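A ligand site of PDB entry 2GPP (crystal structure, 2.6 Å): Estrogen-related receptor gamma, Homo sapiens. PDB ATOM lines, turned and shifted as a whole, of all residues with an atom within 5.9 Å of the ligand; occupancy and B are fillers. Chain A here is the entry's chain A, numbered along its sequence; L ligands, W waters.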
ATOM      1  N   GLU A  19       6.407  27.076 -31.315  1.00  0.00           N
ATOM      2  CA  GLU A  19       6.173  25.663 -31.473  1.00  0.00           C
ATOM      3  C   GLU A  19       4.710  25.412 -31.750  1.00  0.00           C
ATOM      4  O   GLU A  19       3.840  26.171 -31.305  1.00  0.00           O
ATOM      5  CB  GLU A  19       6.585  24.915 -30.234  1.00  0.00           C
ATOM      6  CG  GLU A  19       8.049  25.006 -29.961  1.00  0.00           C
ATOM      7  CD  GLU A  19       8.470  24.158 -28.799  1.00  0.00           C
ATOM      8  OE1 GLU A  19       7.752  23.172 -28.462  1.00  0.00           O
ATOM      9  OE2 GLU A  19       9.520  24.493 -28.213  1.00  0.00           O
ATOM     10  N   LYS A  20       4.466  24.358 -32.516  1.00  0.00           N
ATOM     11  CA  LYS A  20       3.142  23.831 -32.703  1.00  0.00           C
ATOM     12  C   LYS A  20       3.247  22.328 -32.615  1.00  0.00           C
ATOM     13  O   LYS A  20       4.178  21.729 -33.117  1.00  0.00           O
ATOM     14  CB  LYS A  20       2.546  24.287 -34.046  1.00  0.00           C
ATOM     15  CG  LYS A  20       3.314  23.876 -35.296  1.00  0.00           C
ATOM     16  CD  LYS A  20       2.680  24.473 -36.606  1.00  0.00           C
ATOM     17  CE  LYS A  20       3.041  25.972 -36.809  1.00  0.00           C
ATOM     18  NZ  LYS A  20       2.069  26.744 -37.704  1.00  0.00           N
ATOM     19  N   ILE A  21       2.315  21.713 -31.921  1.00  0.00           N
ATOM     20  CA  ILE A  21       2.211  20.273 -31.950  1.00  0.00           C
ATOM     21  C   ILE A  21       0.744  19.888 -31.972  1.00  0.00           C
ATOM     22  O   ILE A  21      -0.077  20.620 -31.448  1.00  0.00           O
ATOM     23  CB  ILE A  21       2.932  19.654 -30.756  1.00  0.00           C
ATOM     24  CG1 ILE A  21       3.270  18.205 -31.056  1.00  0.00           C
ATOM     25  CG2 ILE A  21       2.108  19.804 -29.477  1.00  0.00           C
ATOM     26  CD1 ILE A  21       4.209  17.613 -30.060  1.00  0.00           C
ATOM     27  N   LEU A  40      -1.052  11.641 -24.725  1.00  0.00           N
ATOM     28  CA  LEU A  40      -0.041  12.371 -23.965  1.00  0.00           C
ATOM     29  C   LEU A  40       1.359  11.770 -24.135  1.00  0.00           C
ATOM     30  O   LEU A  40       2.307  12.498 -24.393  1.00  0.00           O
ATOM     31  CB  LEU A  40      -0.420  12.434 -22.479  1.00  0.00           C
ATOM     32  CG  LEU A  40      -1.698  13.201 -22.125  1.00  0.00           C
ATOM     33  CD1 LEU A  40      -1.811  13.359 -20.622  1.00  0.00           C
ATOM     34  CD2 LEU A  40      -1.754  14.545 -22.792  1.00  0.00           C
ATOM     35  N   CYS A  41       1.493  10.458 -23.999  1.00  0.00           N
ATOM     36  CA  CYS A  41       2.799   9.838 -24.179  1.00  0.00           C
ATOM     37  C   CYS A  41       3.321  10.030 -25.586  1.00  0.00           C
ATOM     38  O   CYS A  41       4.503  10.156 -25.790  1.00  0.00           O
ATOM     39  CB  CYS A  41       2.763   8.365 -23.825  1.00  0.00           C
ATOM     40  SG  CYS A  41       2.534   8.071 -22.080  1.00  0.00           S
ATOM     41  N   LEU A  43       2.613  12.652 -27.516  1.00  0.00           N
ATOM     42  CA  LEU A  43       2.990  14.049 -27.558  1.00  0.00           C
ATOM     43  C   LEU A  43       4.306  14.261 -26.878  1.00  0.00           C
ATOM     44  O   LEU A  43       5.159  14.964 -27.363  1.00  0.00           O
ATOM     45  CB  LEU A  43       1.937  14.884 -26.851  1.00  0.00           C
ATOM     46  CG  LEU A  43       0.683  15.071 -27.686  1.00  0.00           C
ATOM     47  CD1 LEU A  43      -0.463  15.500 -26.816  1.00  0.00           C
ATOM     48  CD2 LEU A  43       0.935  16.084 -28.792  1.00  0.00           C
ATOM     49  N   ALA A  44       4.462  13.654 -25.708  1.00  0.00           N
ATOM     50  CA  ALA A  44       5.694  13.740 -24.957  1.00  0.00           C
ATOM     51  C   ALA A  44       6.872  13.238 -25.784  1.00  0.00           C
ATOM     52  O   ALA A  44       7.867  13.926 -25.923  1.00  0.00           O
ATOM     53  CB  ALA A  44       5.578  12.980 -23.695  1.00  0.00           C
ATOM     54  N   GLU A  47       7.574  15.832 -28.618  1.00  0.00           N
ATOM     55  CA  GLU A  47       8.179  17.063 -28.079  1.00  0.00           C
ATOM     56  C   GLU A  47       9.617  16.867 -27.651  1.00  0.00           C
ATOM     57  O   GLU A  47      10.406  17.784 -27.751  1.00  0.00           O
ATOM     58  CB  GLU A  47       7.394  17.625 -26.885  1.00  0.00           C
ATOM     59  CG  GLU A  47       6.514  18.785 -27.196  1.00  0.00           C
ATOM     60  CD  GLU A  47       7.259  19.928 -27.848  1.00  0.00           C
ATOM     61  OE1 GLU A  47       8.093  20.568 -27.183  1.00  0.00           O
ATOM     62  OE2 GLU A  47       7.002  20.201 -29.045  1.00  0.00           O
ATOM     63  N   MET A  78      11.451  16.112 -17.996  1.00  0.00           N
ATOM     64  CA  MET A  78      10.055  16.317 -17.639  1.00  0.00           C
ATOM     65  C   MET A  78       9.809  17.752 -17.231  1.00  0.00           C
ATOM     66  O   MET A  78       8.724  18.280 -17.451  1.00  0.00           O
ATOM     67  CB  MET A  78       9.649  15.378 -16.518  1.00  0.00           C
ATOM     68  CG  MET A  78       8.177  15.401 -16.209  1.00  0.00           C
ATOM     69  SD  MET A  78       7.154  15.071 -17.675  1.00  0.00           S
ATOM     70  CE  MET A  78       7.106  13.298 -17.582  1.00  0.00           C
ATOM     71  N   LEU A  81       9.361  19.534 -20.459  1.00  0.00           N
ATOM     72  CA  LEU A  81       8.068  19.199 -21.036  1.00  0.00           C
ATOM     73  C   LEU A  81       6.963  19.936 -20.324  1.00  0.00           C
ATOM     74  O   LEU A  81       6.131  20.575 -20.938  1.00  0.00           O
ATOM     75  CB  LEU A  81       7.780  17.692 -20.958  1.00  0.00           C
ATOM     76  CG  LEU A  81       8.536  16.831 -21.956  1.00  0.00           C
ATOM     77  CD1 LEU A  81       8.510  15.366 -21.549  1.00  0.00           C
ATOM     78  CD2 LEU A  81       7.950  17.005 -23.324  1.00  0.00           C
ATOM     79  N   ILE A  82       6.962  19.864 -18.999  1.00  0.00           N
ATOM     80  CA  ILE A  82       5.919  20.499 -18.225  1.00  0.00           C
ATOM     81  C   ILE A  82       5.967  21.993 -18.425  1.00  0.00           C
ATOM     82  O   ILE A  82       4.949  22.643 -18.545  1.00  0.00           O
ATOM     83  CB  ILE A  82       6.053  20.174 -16.744  1.00  0.00           C
ATOM     84  CG1 ILE A  82       5.485  18.777 -16.505  1.00  0.00           C
ATOM     85  CG2 ILE A  82       5.300  21.171 -15.895  1.00  0.00           C
ATOM     86  CD1 ILE A  82       5.949  18.186 -15.231  1.00  0.00           C
ATOM     87  N   GLY A  84       6.761  23.635 -20.959  1.00  0.00           N
ATOM     88  CA  GLY A  84       6.205  23.989 -22.252  1.00  0.00           C
ATOM     89  C   GLY A  84       4.700  24.068 -22.174  1.00  0.00           C
ATOM     90  O   GLY A  84       4.079  25.063 -22.554  1.00  0.00           O
ATOM     91  N   VAL A  85       4.120  22.993 -21.655  1.00  0.00           N
ATOM     92  CA  VAL A  85       2.680  22.902 -21.542  1.00  0.00           C
ATOM     93  C   VAL A  85       2.175  24.096 -20.751  1.00  0.00           C
ATOM     94  O   VAL A  85       1.181  24.731 -21.099  1.00  0.00           O
ATOM     95  CB  VAL A  85       2.262  21.612 -20.859  1.00  0.00           C
ATOM     96  CG1 VAL A  85       0.752  21.553 -20.692  1.00  0.00           C
ATOM     97  CG2 VAL A  85       2.699  20.448 -21.682  1.00  0.00           C
ATOM     98  N   ARG A  88       2.106  27.282 -22.883  1.00  0.00           N
ATOM     99  CA  ARG A  88       1.062  27.263 -23.877  1.00  0.00           C
ATOM    100  C   ARG A  88      -0.290  27.500 -23.229  1.00  0.00           C
ATOM    101  O   ARG A  88      -1.208  27.986 -23.884  1.00  0.00           O
ATOM    102  CB  ARG A  88       1.008  25.914 -24.625  1.00  0.00           C
ATOM    103  CG  ARG A  88       2.308  25.384 -25.173  1.00  0.00           C
ATOM    104  CD  ARG A  88       3.090  26.371 -26.010  1.00  0.00           C
ATOM    105  NE  ARG A  88       4.445  25.858 -26.282  1.00  0.00           N
ATOM    106  CZ  ARG A  88       5.439  26.618 -26.724  1.00  0.00           C
ATOM    107  NH1 ARG A  88       5.220  27.913 -26.999  1.00  0.00           N
ATOM    108  NH2 ARG A  88       6.659  26.109 -26.918  1.00  0.00           N
ATOM    109  N   VAL A  97      -2.901  23.017 -22.264  1.00  0.00           N
ATOM    110  CA  VAL A  97      -2.681  22.854 -23.670  1.00  0.00           C
ATOM    111  C   VAL A  97      -1.548  21.869 -23.885  1.00  0.00           C
ATOM    112  O   VAL A  97      -0.383  22.242 -23.937  1.00  0.00           O
ATOM    113  CB  VAL A  97      -2.358  24.182 -24.359  1.00  0.00           C
ATOM    114  CG1 VAL A  97      -2.228  23.999 -25.875  1.00  0.00           C
ATOM    115  CG2 VAL A  97      -3.428  25.250 -24.041  1.00  0.00           C
ATOM    116  N   TYR A  98      -1.888  20.593 -23.993  1.00  0.00           N
ATOM    117  CA  TYR A  98      -0.915  19.562 -24.267  1.00  0.00           C
ATOM    118  C   TYR A  98      -0.563  19.484 -25.745  1.00  0.00           C
ATOM    119  O   TYR A  98       0.501  18.998 -26.122  1.00  0.00           O
ATOM    120  CB  TYR A  98      -1.413  18.234 -23.767  1.00  0.00           C
ATOM    121  CG  TYR A  98      -1.147  18.065 -22.309  1.00  0.00           C
ATOM    122  CD1 TYR A  98       0.140  17.794 -21.863  1.00  0.00           C
ATOM    123  CD2 TYR A  98      -2.160  18.180 -21.367  1.00  0.00           C
ATOM    124  CE1 TYR A  98       0.401  17.619 -20.521  1.00  0.00           C
ATOM    125  CE2 TYR A  98      -1.911  18.009 -20.020  1.00  0.00           C
ATOM    126  CZ  TYR A  98      -0.620  17.729 -19.610  1.00  0.00           C
ATOM    127  OH  TYR A  98      -0.352  17.558 -18.274  1.00  0.00           O
ATOM    128  N   ALA A  99      -1.510  19.939 -26.565  1.00  0.00           N
ATOM    129  CA  ALA A  99      -1.301  20.160 -27.981  1.00  0.00           C
ATOM    130  C   ALA A  99      -2.290  21.246 -28.359  1.00  0.00           C
ATOM    131  O   ALA A  99      -3.213  21.545 -27.597  1.00  0.00           O
ATOM    132  CB  ALA A  99      -1.547  18.874 -28.771  1.00  0.00           C
ATOM    133  N   ASP A 100      -2.087  21.861 -29.524  1.00  0.00           N
ATOM    134  CA  ASP A 100      -3.019  22.884 -29.998  1.00  0.00           C
ATOM    135  C   ASP A 100      -4.394  22.316 -30.226  1.00  0.00           C
ATOM    136  O   ASP A 100      -5.364  23.034 -30.096  1.00  0.00           O
ATOM    137  CB  ASP A 100      -2.506  23.535 -31.272  1.00  0.00           C
ATOM    138  CG  ASP A 100      -1.341  24.444 -31.020  1.00  0.00           C
ATOM    139  OD1 ASP A 100      -1.144  24.816 -29.837  1.00  0.00           O
ATOM    140  OD2 ASP A 100      -0.603  24.770 -31.970  1.00  0.00           O
ATOM    141  N   LEU A 117      -2.124  15.561 -10.913  1.00  0.00           N
ATOM    142  CA  LEU A 117      -1.017  16.078 -11.699  1.00  0.00           C
ATOM    143  C   LEU A 117      -1.325  17.381 -12.434  1.00  0.00           C
ATOM    144  O   LEU A 117      -0.519  18.322 -12.406  1.00  0.00           O
ATOM    145  CB  LEU A 117      -0.531  15.041 -12.705  1.00  0.00           C
ATOM    146  CG  LEU A 117       0.556  15.577 -13.644  1.00  0.00           C
ATOM    147  CD1 LEU A 117       1.785  16.030 -12.853  1.00  0.00           C
ATOM    148  CD2 LEU A 117       0.938  14.549 -14.689  1.00  0.00           C
ATOM    149  N   ILE A 121       0.140  21.369 -12.222  1.00  0.00           N
ATOM    150  CA  ILE A 121       0.582  22.109 -13.401  1.00  0.00           C
ATOM    151  C   ILE A 121      -0.144  23.454 -13.493  1.00  0.00           C
ATOM    152  O   ILE A 121       0.478  24.478 -13.800  1.00  0.00           O
ATOM    153  CB  ILE A 121       0.377  21.293 -14.675  1.00  0.00           C
ATOM    154  CG1 ILE A 121       1.313  20.077 -14.668  1.00  0.00           C
ATOM    155  CG2 ILE A 121       0.672  22.122 -15.873  1.00  0.00           C
ATOM    156  CD1 ILE A 121       0.917  18.967 -15.579  1.00  0.00           C
ATOM    157  N   ALA A 203       5.031  13.845 -12.022  1.00  0.00           N
ATOM    158  CA  ALA A 203       4.702  13.372 -13.358  1.00  0.00           C
ATOM    159  C   ALA A 203       5.465  12.117 -13.721  1.00  0.00           C
ATOM    160  O   ALA A 203       4.879  11.174 -14.228  1.00  0.00           O
ATOM    161  CB  ALA A 203       4.968  14.441 -14.371  1.00  0.00           C
ATOM    162  N   PHE A 207       3.865   8.442 -14.451  1.00  0.00           N
ATOM    163  CA  PHE A 207       3.963   7.832 -15.759  1.00  0.00           C
ATOM    164  C   PHE A 207       4.851   6.611 -15.745  1.00  0.00           C
ATOM    165  O   PHE A 207       4.768   5.749 -16.614  1.00  0.00           O
ATOM    166  CB  PHE A 207       4.408   8.852 -16.809  1.00  0.00           C
ATOM    167  CG  PHE A 207       3.262   9.590 -17.420  1.00  0.00           C
ATOM    168  CD1 PHE A 207       2.704  10.669 -16.776  1.00  0.00           C
ATOM    169  CD2 PHE A 207       2.677   9.148 -18.582  1.00  0.00           C
ATOM    170  CE1 PHE A 207       1.637  11.315 -17.315  1.00  0.00           C
ATOM    171  CE2 PHE A 207       1.607   9.804 -19.135  1.00  0.00           C
ATOM    172  CZ  PHE A 207       1.079  10.877 -18.493  1.00  0.00           C
ATOM    173  N   PHE A 222      10.487   8.275 -25.279  1.00  0.00           N
ATOM    174  CA  PHE A 222       9.795   8.511 -24.036  1.00  0.00           C
ATOM    175  C   PHE A 222      10.164   7.447 -22.985  1.00  0.00           C
ATOM    176  O   PHE A 222      10.350   7.777 -21.829  1.00  0.00           O
ATOM    177  CB  PHE A 222       8.271   8.572 -24.279  1.00  0.00           C
ATOM    178  CG  PHE A 222       7.465   8.903 -23.063  1.00  0.00           C
ATOM    179  CD1 PHE A 222       7.344  10.202 -22.644  1.00  0.00           C
ATOM    180  CD2 PHE A 222       6.850   7.928 -22.341  1.00  0.00           C
ATOM    181  CE1 PHE A 222       6.624  10.523 -21.536  1.00  0.00           C
ATOM    182  CE2 PHE A 222       6.106   8.246 -21.230  1.00  0.00           C
ATOM    183  CZ  PHE A 222       6.007   9.557 -20.828  1.00  0.00           C
HETATM  184  N1  LIG L   1       3.733  19.151 -24.397  1.00  0.00           N
HETATM  185  C1  LIG L   1       3.682  15.365 -20.948  1.00  0.00           C
HETATM  186  C2  LIG L   1       2.964  14.964 -22.058  1.00  0.00           C
HETATM  187  C3  LIG L   1       2.847  15.815 -23.131  1.00  0.00           C
HETATM  188  C4  LIG L   1       3.426  17.064 -23.106  1.00  0.00           C
HETATM  189  C5  LIG L   1       3.253  17.949 -24.279  1.00  0.00           C
HETATM  190  C6  LIG L   1       3.259  21.905 -26.767  1.00  0.00           C
HETATM  191  C7  LIG L   1       2.146  23.481 -28.656  1.00  0.00           C
HETATM  192  C8  LIG L   1       4.052  22.435 -27.750  1.00  0.00           C
HETATM  193  C9  LIG L   1       4.247  16.618 -20.940  1.00  0.00           C
HETATM  194  C10 LIG L   1       2.992  14.894 -18.591  1.00  0.00           C
HETATM  195  C11 LIG L   1       3.894  14.515 -19.737  1.00  0.00           C
HETATM  196  C12 LIG L   1       3.743  13.041 -20.043  1.00  0.00           C
HETATM  197  N2  LIG L   1       3.434  19.780 -25.575  1.00  0.00           N
HETATM  198  C13 LIG L   1       3.904  21.066 -25.753  1.00  0.00           C
HETATM  199  O1  LIG L   1       4.809  21.584 -25.135  1.00  0.00           O
HETATM  200  C14 LIG L   1       1.900  22.159 -26.716  1.00  0.00           C
HETATM  201  C15 LIG L   1       1.335  22.964 -27.668  1.00  0.00           C
HETATM  202  O2  LIG L   1       1.598  24.296 -29.633  1.00  0.00           O
HETATM  203  C16 LIG L   1       3.494  23.233 -28.715  1.00  0.00           C
HETATM  204  C17 LIG L   1       4.125  17.477 -22.013  1.00  0.00           C
HETATM  205  O   HOH W   1       5.799  23.819 -25.363  1.00  0.00           O
HETATM  206  O   HOH W   2       6.390  20.508 -23.517  1.00  0.00           O
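The side-chain carboxylate (OD1) of Asp 100 lies within hydrogen-bond range of an oxygen (O2) of the ligand (2.8 Å).
An oxygen (O2) of the ligand sits at hydrogen-bond distance from the backbone carbonyl oxygen of Glu 19 (3.4 Å).
The backbone carbonyl oxygen (O) of Tyr 98 is in hydrogen-bond range of a nitrogen (N2) of the ligand, 3.1 Å away.
NH2 of Arg 88 lies within salt-bridge range of OE1 of Glu 19 (3.5 Å).
The backbone NH (N) of Asp 100 lies within hydrogen-bond range of the backbone carbonyl oxygen (O) of Ile 21, at 3.0 Å.
Residues that only touch the ligand: Lys 20, Ile 21, Leu 40, Leu 43, Ala 44, Glu 47, Met 78, Leu 81, Gly 84, Val 85, Arg 88, Val 97, Ala 99 and Phe 207.
Hydrophobic or aromatic side chains within 4 Å of the ligand: Ile 21, Leu 43, Ala 44, Met 78, Leu 81, Val 85, Tyr 98 and Phe 207.
17 residues have an atom within 4 Å of the ligand: Glu 19, Lys 20, Ile 21, Leu 40, Leu 43, Ala 44, Glu 47, Met 78, Leu 81, Gly 84, Val 85, Arg 88, Val 97, Tyr 98, Ala 99, Asp 100 and Phe 207.
The nearest printed residue that does not touch the ligand is Phe 222 (4.1 Å).
Water W1 bridges an oxygen (O1) of the ligand (2.5 Å) and the guanidinium group (NE) of Arg 88 (2.6 Å).
Water W2 bridges an oxygen (O1) of the ligand (2.5 Å) and the backbone carbonyl oxygen (O) of Leu 81 (2.6 Å).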
